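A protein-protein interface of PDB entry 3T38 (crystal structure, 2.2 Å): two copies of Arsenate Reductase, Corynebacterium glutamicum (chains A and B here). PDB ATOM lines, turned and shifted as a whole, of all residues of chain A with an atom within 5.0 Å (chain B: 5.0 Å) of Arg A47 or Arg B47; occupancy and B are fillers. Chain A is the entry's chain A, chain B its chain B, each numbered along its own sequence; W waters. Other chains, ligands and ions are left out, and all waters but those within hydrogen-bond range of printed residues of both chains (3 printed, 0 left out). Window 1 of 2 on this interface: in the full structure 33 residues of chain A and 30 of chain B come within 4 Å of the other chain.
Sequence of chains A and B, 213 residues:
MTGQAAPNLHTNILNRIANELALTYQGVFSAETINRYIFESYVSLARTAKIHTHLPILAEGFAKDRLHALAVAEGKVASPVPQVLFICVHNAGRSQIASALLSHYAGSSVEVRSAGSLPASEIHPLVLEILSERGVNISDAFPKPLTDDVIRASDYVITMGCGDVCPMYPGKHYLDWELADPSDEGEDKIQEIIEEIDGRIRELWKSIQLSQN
Of chain B, only Arg B47, Gly B116, Ser B117, Pro B145, Leu B146 and Val B165 come within 4 Å of Arg A47.
Of the printed residues of chain B, Ser A117 touches Arg B47 (3.3 Å).
Printed residues of chain A within 4 Å of Val B43: Leu A146 (3.6 Å).
Arg B47 touches just these residues of chain A: Arg A47 (3.3 Å), Gly A116 (3.6 Å), Ser A117 (3.3 Å), Leu A118 (3.9 Å), Pro A145 (3.5 Å), Leu A146 (3.4 Å) and Val A165 (3.8 Å).
Of the printed residues of chain A, Thr B48 touches Leu A118.
Ala B49 touches none of the printed residues of chain A.
Of the printed residues of chain A, Ser B117 touches Arg A47 (3.5 Å).
The nearest residue of chain A that does not touch Arg B47 is Pro A119 (4.7 Å).
O of Ser A117 is in hydrogen-bond range of NH1 of Arg B47, at 3.3 Å.
The guanidinium group of Arg A47 lies close to the guanidinium group of Arg B47 (3.3 Å).
The guanidinium group (NH1) of Arg A47 lies within hydrogen-bond range of the backbone carbonyl oxygen (O) of Leu B146 (2.7 Å).
O of Leu A146 sits close to NE of Arg B47 (3.4 Å).
Among the printed residues, merely in contact across the chains: Val A43 with Leu B146 (3.4 Å), Val A165 with Ala B46 (3.4 Å), Arg A47 with Ser B117 (3.5 Å), Leu A118 with Thr B48 (3.5 Å), Ala A46 with Val B165 (3.5 Å), Arg A47 with Pro B145 (3.5 Å), Pro A145 with Arg B47 (3.5 Å), Leu A146 with Val B43 (3.6 Å), Gly A116 with Arg B47 (3.6 Å), Arg A47 with Gly B116 (3.7 Å), Val A165 with Lys B50 (3.7 Å), Arg A47 with Val B165 (3.8 Å), Val A43 with Thr B147 (3.8 Å), Val A165 with Arg B47 (3.8 Å), Leu A118 with Arg B47 (3.9 Å) and Thr A48 with Leu B118 (3.9 Å).
Val A43 touches Leu B146, and with the chains exchanged Leu A146 touches Val B43.
Ala A46 touches Val B165, and with the chains exchanged Val A165 touches Ala B46.
Arg A47 touches its own counterpart, Arg B47.
Thr A48 touches Leu B118, and with the chains exchanged Leu A118 touches Thr B48.
14 positions are printed for both chains.
Of the 20 pairs that touch across the chains among the printed residues, 17 have their exchanged pair printed and touching as well.
Of the 15 printed residues of chain A, 10 touch a printed residue of chain B.
Hydrophobic or aromatic side chains of chain A that line the printed part of chain B: Val A43, Ala A46, Leu A118, Pro A145, Leu A146 and Val A165.
Of the 15 printed residues of chain B, 12 touch a printed residue of chain A.
Hydrophobic or aromatic side chains of chain B within 4 Å of the printed part of chain A: Val B43, Ala B46, Leu B118, Pro B145, Leu B146 and Val B165.
Among the printed residues, no Asp or Glu carboxylate lies within 4 Å of a Lys or Arg side-chain nitrogen of the other chain.
Water W3 bridges OG of Ser A117 (2.5 Å) and NZ of Lys B50 (3.0 Å).
Water W1 bridges O of Ser B117 (2.5 Å) and NE of Arg A47 (2.9 Å).
Water W2 lies within hydrogen-bond range of NH2 of Arg A47 (2.8 Å) and NH1 of Arg B47 (3.2 Å).
The backbone carbonyl oxygen of Gly B116 sits at hydrogen-bond distance from the backbone NH of Leu B146.
The backbone NH (N) of Leu A146 lies within hydrogen-bond range of the backbone carbonyl oxygen (O) of Gly A116.
O of Leu A45 is in hydrogen-bond range of OG1 of Thr A48 (3.4 Å).
O of Arg B47 lies within hydrogen-bond range of NZ of Lys B50 (2.7 Å).
The side-chain hydroxyl of Ser B44 sits at hydrogen-bond distance from the guanidinium group of Arg B47 (2.9 Å).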
ATOM      1  N   VAL A  43      -4.625  18.106  19.405  1.00  0.00           N
ATOM      2  CA  VAL A  43      -3.710  16.991  19.385  1.00  0.00           C
ATOM      3  C   VAL A  43      -4.407  15.732  19.797  1.00  0.00           C
ATOM      4  O   VAL A  43      -4.303  14.703  19.052  1.00  0.00           O
ATOM      5  CB  VAL A  43      -2.366  17.260  20.144  1.00  0.00           C
ATOM      6  CG1 VAL A  43      -1.559  15.945  20.243  1.00  0.00           C
ATOM      7  CG2 VAL A  43      -1.536  18.299  19.374  1.00  0.00           C
ATOM      8  N   SER A  44      -5.210  15.807  20.864  1.00  0.00           N
ATOM      9  CA  SER A  44      -6.076  14.667  21.230  1.00  0.00           C
ATOM     10  C   SER A  44      -6.883  14.104  20.072  1.00  0.00           C
ATOM     11  O   SER A  44      -6.930  12.869  19.837  1.00  0.00           O
ATOM     12  CB  SER A  44      -7.051  15.082  22.343  1.00  0.00           C
ATOM     13  OG  SER A  44      -6.231  15.124  23.516  1.00  0.00           O
ATOM     14  N   LEU A  45      -7.564  14.999  19.363  1.00  0.00           N
ATOM     15  CA  LEU A  45      -8.394  14.508  18.252  1.00  0.00           C
ATOM     16  C   LEU A  45      -7.544  14.016  17.122  1.00  0.00           C
ATOM     17  O   LEU A  45      -7.907  13.028  16.423  1.00  0.00           O
ATOM     18  CB  LEU A  45      -9.383  15.586  17.808  1.00  0.00           C
ATOM     19  CG  LEU A  45     -10.477  15.879  18.880  1.00  0.00           C
ATOM     20  CD1 LEU A  45     -11.317  17.065  18.398  1.00  0.00           C
ATOM     21  CD2 LEU A  45     -11.359  14.679  19.102  1.00  0.00           C
ATOM     22  N   ALA A  46      -6.391  14.689  16.912  1.00  0.00           N
ATOM     23  CA  ALA A  46      -5.532  14.314  15.797  1.00  0.00           C
ATOM     24  C   ALA A  46      -5.051  12.884  15.935  1.00  0.00           C
ATOM     25  O   ALA A  46      -4.822  12.202  14.941  1.00  0.00           O
ATOM     26  CB  ALA A  46      -4.360  15.242  15.700  1.00  0.00           C
ATOM     27  N   ARG A  47      -4.887  12.426  17.175  1.00  0.00           N
ATOM     28  CA  ARG A  47      -4.350  11.067  17.431  1.00  0.00           C
ATOM     29  C   ARG A  47      -5.203   9.977  16.813  1.00  0.00           C
ATOM     30  O   ARG A  47      -4.662   8.991  16.280  1.00  0.00           O
ATOM     31  CB  ARG A  47      -4.183  10.843  18.931  1.00  0.00           C
ATOM     32  CG  ARG A  47      -2.931  11.530  19.504  1.00  0.00           C
ATOM     33  CD  ARG A  47      -2.630  11.063  20.963  1.00  0.00           C
ATOM     34  NE  ARG A  47      -3.883  10.961  21.701  1.00  0.00           N
ATOM     35  CZ  ARG A  47      -4.262  11.755  22.699  1.00  0.00           C
ATOM     36  NH1 ARG A  47      -3.507  12.807  23.136  1.00  0.00           N
ATOM     37  NH2 ARG A  47      -5.431  11.500  23.260  1.00  0.00           N
ATOM     38  N   THR A  48      -6.522  10.178  16.843  1.00  0.00           N
ATOM     39  CA  THR A  48      -7.466   9.124  16.427  1.00  0.00           C
ATOM     40  C   THR A  48      -8.087   9.437  15.086  1.00  0.00           C
ATOM     41  O   THR A  48      -8.421   8.530  14.344  1.00  0.00           O
ATOM     42  CB  THR A  48      -8.605   8.900  17.471  1.00  0.00           C
ATOM     43  OG1 THR A  48      -9.105  10.173  17.906  1.00  0.00           O
ATOM     44  CG2 THR A  48      -8.016   8.162  18.714  1.00  0.00           C
ATOM     45  N   ALA A  49      -8.232  10.724  14.792  1.00  0.00           N
ATOM     46  CA  ALA A  49      -8.967  11.175  13.606  1.00  0.00           C
ATOM     47  C   ALA A  49      -8.015  11.466  12.488  1.00  0.00           C
ATOM     48  O   ALA A  49      -8.408  11.389  11.359  1.00  0.00           O
ATOM     49  CB  ALA A  49      -9.849  12.446  13.928  1.00  0.00           C
ATOM     50  N   LYS A  50      -6.755  11.739  12.808  1.00  0.00           N
ATOM     51  CA  LYS A  50      -5.712  12.210  11.857  1.00  0.00           C
ATOM     52  C   LYS A  50      -5.900  13.712  11.538  1.00  0.00           C
ATOM     53  O   LYS A  50      -6.992  14.263  11.766  1.00  0.00           O
ATOM     54  CB  LYS A  50      -5.628  11.343  10.562  1.00  0.00           C
ATOM     55  CG  LYS A  50      -6.571  11.804   9.376  1.00  0.00           C
ATOM     56  CD  LYS A  50      -6.631  10.826   8.161  1.00  0.00           C
ATOM     57  CE  LYS A  50      -5.861  11.390   6.919  1.00  0.00           C
ATOM     58  NZ  LYS A  50      -4.364  11.632   7.060  1.00  0.00           N
ATOM     59  N   GLY A 116     -15.064   8.470  24.687  1.00  0.00           N
ATOM     60  CA  GLY A 116     -14.569   7.130  24.494  1.00  0.00           C
ATOM     61  C   GLY A 116     -13.251   6.954  25.217  1.00  0.00           C
ATOM     62  O   GLY A 116     -12.541   7.944  25.479  1.00  0.00           O
ATOM     63  N   SER A 117     -12.968   5.714  25.619  1.00  0.00           N
ATOM     64  CA  SER A 117     -11.631   5.357  26.073  1.00  0.00           C
ATOM     65  C   SER A 117     -10.683   5.278  24.846  1.00  0.00           C
ATOM     66  O   SER A 117      -9.484   5.556  24.958  1.00  0.00           O
ATOM     67  CB  SER A 117     -11.653   4.039  26.871  1.00  0.00           C
ATOM     68  OG  SER A 117     -12.069   2.947  26.074  1.00  0.00           O
ATOM     69  N   LEU A 118     -11.187   4.793  23.713  1.00  0.00           N
ATOM     70  CA  LEU A 118     -10.313   4.584  22.553  1.00  0.00           C
ATOM     71  C   LEU A 118     -11.064   5.052  21.276  1.00  0.00           C
ATOM     72  O   LEU A 118     -11.536   4.236  20.445  1.00  0.00           O
ATOM     73  CB  LEU A 118      -9.941   3.099  22.439  1.00  0.00           C
ATOM     74  CG  LEU A 118      -9.332   2.358  23.637  1.00  0.00           C
ATOM     75  CD1 LEU A 118      -9.245   0.745  23.370  1.00  0.00           C
ATOM     76  CD2 LEU A 118      -7.934   2.921  24.111  1.00  0.00           C
ATOM     77  N   PRO A 119     -11.208   6.368  21.129  1.00  0.00           N
ATOM     78  CA  PRO A 119     -12.066   6.874  20.048  1.00  0.00           C
ATOM     79  C   PRO A 119     -11.771   6.305  18.678  1.00  0.00           C
ATOM     80  O   PRO A 119     -10.642   6.231  18.268  1.00  0.00           O
ATOM     81  CB  PRO A 119     -11.773   8.383  20.046  1.00  0.00           C
ATOM     82  CG  PRO A 119     -11.347   8.692  21.488  1.00  0.00           C
ATOM     83  CD  PRO A 119     -10.568   7.446  21.929  1.00  0.00           C
ATOM     84  N   PRO A 145     -11.908  11.582  23.086  1.00  0.00           N
ATOM     85  CA  PRO A 145     -11.558  10.836  24.300  1.00  0.00           C
ATOM     86  C   PRO A 145     -12.189  11.376  25.559  1.00  0.00           C
ATOM     87  O   PRO A 145     -12.388  12.604  25.723  1.00  0.00           O
ATOM     88  CB  PRO A 145     -10.043  11.039  24.426  1.00  0.00           C
ATOM     89  CG  PRO A 145      -9.782  12.479  23.855  1.00  0.00           C
ATOM     90  CD  PRO A 145     -10.937  12.667  22.768  1.00  0.00           C
ATOM     91  N   LEU A 146     -12.410  10.463  26.502  1.00  0.00           N
ATOM     92  CA  LEU A 146     -12.741  10.845  27.870  1.00  0.00           C
ATOM     93  C   LEU A 146     -11.741  11.828  28.475  1.00  0.00           C
ATOM     94  O   LEU A 146     -10.542  11.631  28.397  1.00  0.00           O
ATOM     95  CB  LEU A 146     -12.777   9.592  28.739  1.00  0.00           C
ATOM     96  CG  LEU A 146     -13.330   9.795  30.138  1.00  0.00           C
ATOM     97  CD1 LEU A 146     -14.814  10.412  30.082  1.00  0.00           C
ATOM     98  CD2 LEU A 146     -13.223   8.367  30.774  1.00  0.00           C
ATOM     99  N   VAL A 165     -12.018   2.857  33.437  1.00  0.00           N
ATOM    100  CA  VAL A 165     -11.168   3.964  32.972  1.00  0.00           C
ATOM    101  C   VAL A 165     -11.572   5.314  33.580  1.00  0.00           C
ATOM    102  O   VAL A 165     -10.982   6.353  33.239  1.00  0.00           O
ATOM    103  CB  VAL A 165     -11.241   4.158  31.449  1.00  0.00           C
ATOM    104  CG1 VAL A 165     -10.723   2.894  30.676  1.00  0.00           C
ATOM    105  CG2 VAL A 165     -12.659   4.578  31.054  1.00  0.00           C
ATOM    106  N   VAL B  43      -6.385  10.806  33.738  1.00  0.00           N
ATOM    107  CA  VAL B  43      -7.492  10.267  32.953  1.00  0.00           C
ATOM    108  C   VAL B  43      -7.024   9.842  31.589  1.00  0.00           C
ATOM    109  O   VAL B  43      -7.472   8.828  31.029  1.00  0.00           O
ATOM    110  CB  VAL B  43      -8.689  11.224  32.879  1.00  0.00           C
ATOM    111  CG1 VAL B  43      -9.703  10.806  31.838  1.00  0.00           C
ATOM    112  CG2 VAL B  43      -9.455  11.110  34.164  1.00  0.00           C
ATOM    113  N   SER B  44      -6.061  10.568  31.069  1.00  0.00           N
ATOM    114  CA  SER B  44      -5.592  10.300  29.745  1.00  0.00           C
ATOM    115  C   SER B  44      -4.927   8.937  29.673  1.00  0.00           C
ATOM    116  O   SER B  44      -5.120   8.224  28.724  1.00  0.00           O
ATOM    117  CB  SER B  44      -4.551  11.340  29.377  1.00  0.00           C
ATOM    118  OG  SER B  44      -4.579  11.505  28.007  1.00  0.00           O
ATOM    119  N   LEU B  45      -4.066   8.646  30.645  1.00  0.00           N
ATOM    120  CA  LEU B  45      -3.435   7.350  30.734  1.00  0.00           C
ATOM    121  C   LEU B  45      -4.403   6.238  31.178  1.00  0.00           C
ATOM    122  O   LEU B  45      -4.316   5.128  30.651  1.00  0.00           O
ATOM    123  CB  LEU B  45      -2.240   7.408  31.703  1.00  0.00           C
ATOM    124  CG  LEU B  45      -1.002   8.255  31.378  1.00  0.00           C
ATOM    125  CD1 LEU B  45      -0.107   8.323  32.599  1.00  0.00           C
ATOM    126  CD2 LEU B  45      -0.276   7.559  30.218  1.00  0.00           C
ATOM    127  N   ALA B  46      -5.278   6.500  32.170  1.00  0.00           N
ATOM    128  CA  ALA B  46      -6.359   5.541  32.485  1.00  0.00           C
ATOM    129  C   ALA B  46      -7.089   4.997  31.236  1.00  0.00           C
ATOM    130  O   ALA B  46      -7.457   3.816  31.192  1.00  0.00           O
ATOM    131  CB  ALA B  46      -7.384   6.171  33.437  1.00  0.00           C
ATOM    132  N   ARG B  47      -7.331   5.851  30.234  1.00  0.00           N
ATOM    133  CA  ARG B  47      -8.056   5.417  29.022  1.00  0.00           C
ATOM    134  C   ARG B  47      -7.398   4.165  28.396  1.00  0.00           C
ATOM    135  O   ARG B  47      -8.089   3.260  27.953  1.00  0.00           O
ATOM    136  CB  ARG B  47      -8.182   6.536  27.965  1.00  0.00           C
ATOM    137  CG  ARG B  47      -9.214   7.650  28.309  1.00  0.00           C
ATOM    138  CD  ARG B  47      -9.412   8.710  27.182  1.00  0.00           C
ATOM    139  NE  ARG B  47      -8.229   9.542  27.021  1.00  0.00           N
ATOM    140  CZ  ARG B  47      -7.274   9.250  26.170  1.00  0.00           C
ATOM    141  NH1 ARG B  47      -7.442   8.167  25.387  1.00  0.00           N
ATOM    142  NH2 ARG B  47      -6.196  10.027  26.081  1.00  0.00           N
ATOM    143  N   THR B  48      -6.066   4.100  28.393  1.00  0.00           N
ATOM    144  CA  THR B  48      -5.417   2.959  27.729  1.00  0.00           C
ATOM    145  C   THR B  48      -4.784   1.927  28.654  1.00  0.00           C
ATOM    146  O   THR B  48      -4.679   0.749  28.271  1.00  0.00           O
ATOM    147  CB  THR B  48      -4.361   3.419  26.704  1.00  0.00           C
ATOM    148  OG1 THR B  48      -3.440   4.300  27.350  1.00  0.00           O
ATOM    149  CG2 THR B  48      -5.029   4.161  25.569  1.00  0.00           C
ATOM    150  N   ALA B  49      -4.338   2.379  29.833  1.00  0.00           N
ATOM    151  CA  ALA B  49      -3.754   1.501  30.859  1.00  0.00           C
ATOM    152  C   ALA B  49      -4.797   0.972  31.867  1.00  0.00           C
ATOM    153  O   ALA B  49      -4.528  -0.007  32.561  1.00  0.00           O
ATOM    154  CB  ALA B  49      -2.592   2.209  31.575  1.00  0.00           C
ATOM    155  N   LYS B  50      -6.004   1.580  31.894  1.00  0.00           N
ATOM    156  CA  LYS B  50      -7.033   1.315  32.927  1.00  0.00           C
ATOM    157  C   LYS B  50      -6.563   1.839  34.293  1.00  0.00           C
ATOM    158  O   LYS B  50      -5.366   2.087  34.491  1.00  0.00           O
ATOM    159  CB  LYS B  50      -7.459  -0.200  32.988  1.00  0.00           C
ATOM    160  CG  LYS B  50      -8.474  -0.669  31.878  1.00  0.00           C
ATOM    161  CD  LYS B  50      -8.074  -0.178  30.460  1.00  0.00           C
ATOM    162  CE  LYS B  50      -9.210  -0.258  29.387  1.00  0.00           C
ATOM    163  NZ  LYS B  50      -8.984   0.766  28.222  1.00  0.00           N
ATOM    164  N   GLY B 116       2.712   7.833  21.655  1.00  0.00           N
ATOM    165  CA  GLY B 116       1.933   7.107  20.637  1.00  0.00           C
ATOM    166  C   GLY B 116       0.651   7.791  20.208  1.00  0.00           C
ATOM    167  O   GLY B 116       0.147   8.685  20.891  1.00  0.00           O
ATOM    168  N   SER B 117       0.138   7.414  19.052  1.00  0.00           N
ATOM    169  CA  SER B 117      -1.150   7.946  18.625  1.00  0.00           C
ATOM    170  C   SER B 117      -2.241   7.070  19.267  1.00  0.00           C
ATOM    171  O   SER B 117      -3.290   7.566  19.637  1.00  0.00           O
ATOM    172  CB  SER B 117      -1.238   7.881  17.107  1.00  0.00           C
ATOM    173  OG  SER B 117      -0.931   6.534  16.664  1.00  0.00           O
ATOM    174  N   LEU B 118      -1.956   5.764  19.395  1.00  0.00           N
ATOM    175  CA  LEU B 118      -2.865   4.771  19.953  1.00  0.00           C
ATOM    176  C   LEU B 118      -2.099   3.875  20.953  1.00  0.00           C
ATOM    177  O   LEU B 118      -1.697   2.699  20.621  1.00  0.00           O
ATOM    178  CB  LEU B 118      -3.463   3.924  18.829  1.00  0.00           C
ATOM    179  CG  LEU B 118      -4.142   4.632  17.655  1.00  0.00           C
ATOM    180  CD1 LEU B 118      -4.402   3.598  16.528  1.00  0.00           C
ATOM    181  CD2 LEU B 118      -5.478   5.310  18.103  1.00  0.00           C
ATOM    182  N   PRO B 145       0.047   8.992  25.501  1.00  0.00           N
ATOM    183  CA  PRO B 145      -0.427   9.596  24.252  1.00  0.00           C
ATOM    184  C   PRO B 145       0.410  10.757  23.854  1.00  0.00           C
ATOM    185  O   PRO B 145       0.858  11.543  24.713  1.00  0.00           O
ATOM    186  CB  PRO B 145      -1.843  10.123  24.615  1.00  0.00           C
ATOM    187  CG  PRO B 145      -1.809  10.290  26.149  1.00  0.00           C
ATOM    188  CD  PRO B 145      -0.931   9.142  26.601  1.00  0.00           C
ATOM    189  N   LEU B 146       0.507  10.954  22.561  1.00  0.00           N
ATOM    190  CA  LEU B 146       1.033  12.202  22.033  1.00  0.00           C
ATOM    191  C   LEU B 146       0.259  13.417  22.568  1.00  0.00           C
ATOM    192  O   LEU B 146      -0.989  13.443  22.517  1.00  0.00           O
ATOM    193  CB  LEU B 146       0.980  12.177  20.499  1.00  0.00           C
ATOM    194  CG  LEU B 146       1.644  13.341  19.759  1.00  0.00           C
ATOM    195  CD1 LEU B 146       3.223  13.395  20.047  1.00  0.00           C
ATOM    196  CD2 LEU B 146       1.288  13.280  18.261  1.00  0.00           C
ATOM    197  N   THR B 147       0.991  14.444  23.007  1.00  0.00           N
ATOM    198  CA  THR B 147       0.392  15.667  23.495  1.00  0.00           C
ATOM    199  C   THR B 147       1.025  16.882  22.817  1.00  0.00           C
ATOM    200  O   THR B 147       2.115  16.804  22.244  1.00  0.00           O
ATOM    201  CB  THR B 147       0.603  15.802  24.984  1.00  0.00           C
ATOM    202  OG1 THR B 147       1.997  15.531  25.277  1.00  0.00           O
ATOM    203  CG2 THR B 147      -0.304  14.835  25.776  1.00  0.00           C
ATOM    204  N   VAL B 165      -0.490  12.532  12.465  1.00  0.00           N
ATOM    205  CA  VAL B 165      -1.083  12.830  13.774  1.00  0.00           C
ATOM    206  C   VAL B 165      -0.400  14.037  14.443  1.00  0.00           C
ATOM    207  O   VAL B 165      -0.794  14.498  15.532  1.00  0.00           O
ATOM    208  CB  VAL B 165      -1.020  11.611  14.718  1.00  0.00           C
ATOM    209  CG1 VAL B 165      -1.918  10.450  14.164  1.00  0.00           C
ATOM    210  CG2 VAL B 165       0.408  11.164  14.889  1.00  0.00           C
HETATM  211  O   HOH W   1      -4.813   8.199  21.509  1.00  0.00           O
HETATM  212  O   HOH W   2      -7.407   9.697  22.532  1.00  0.00           O
HETATM  213  O   HOH W   3     -11.692   0.724  27.043  1.00  0.00           O
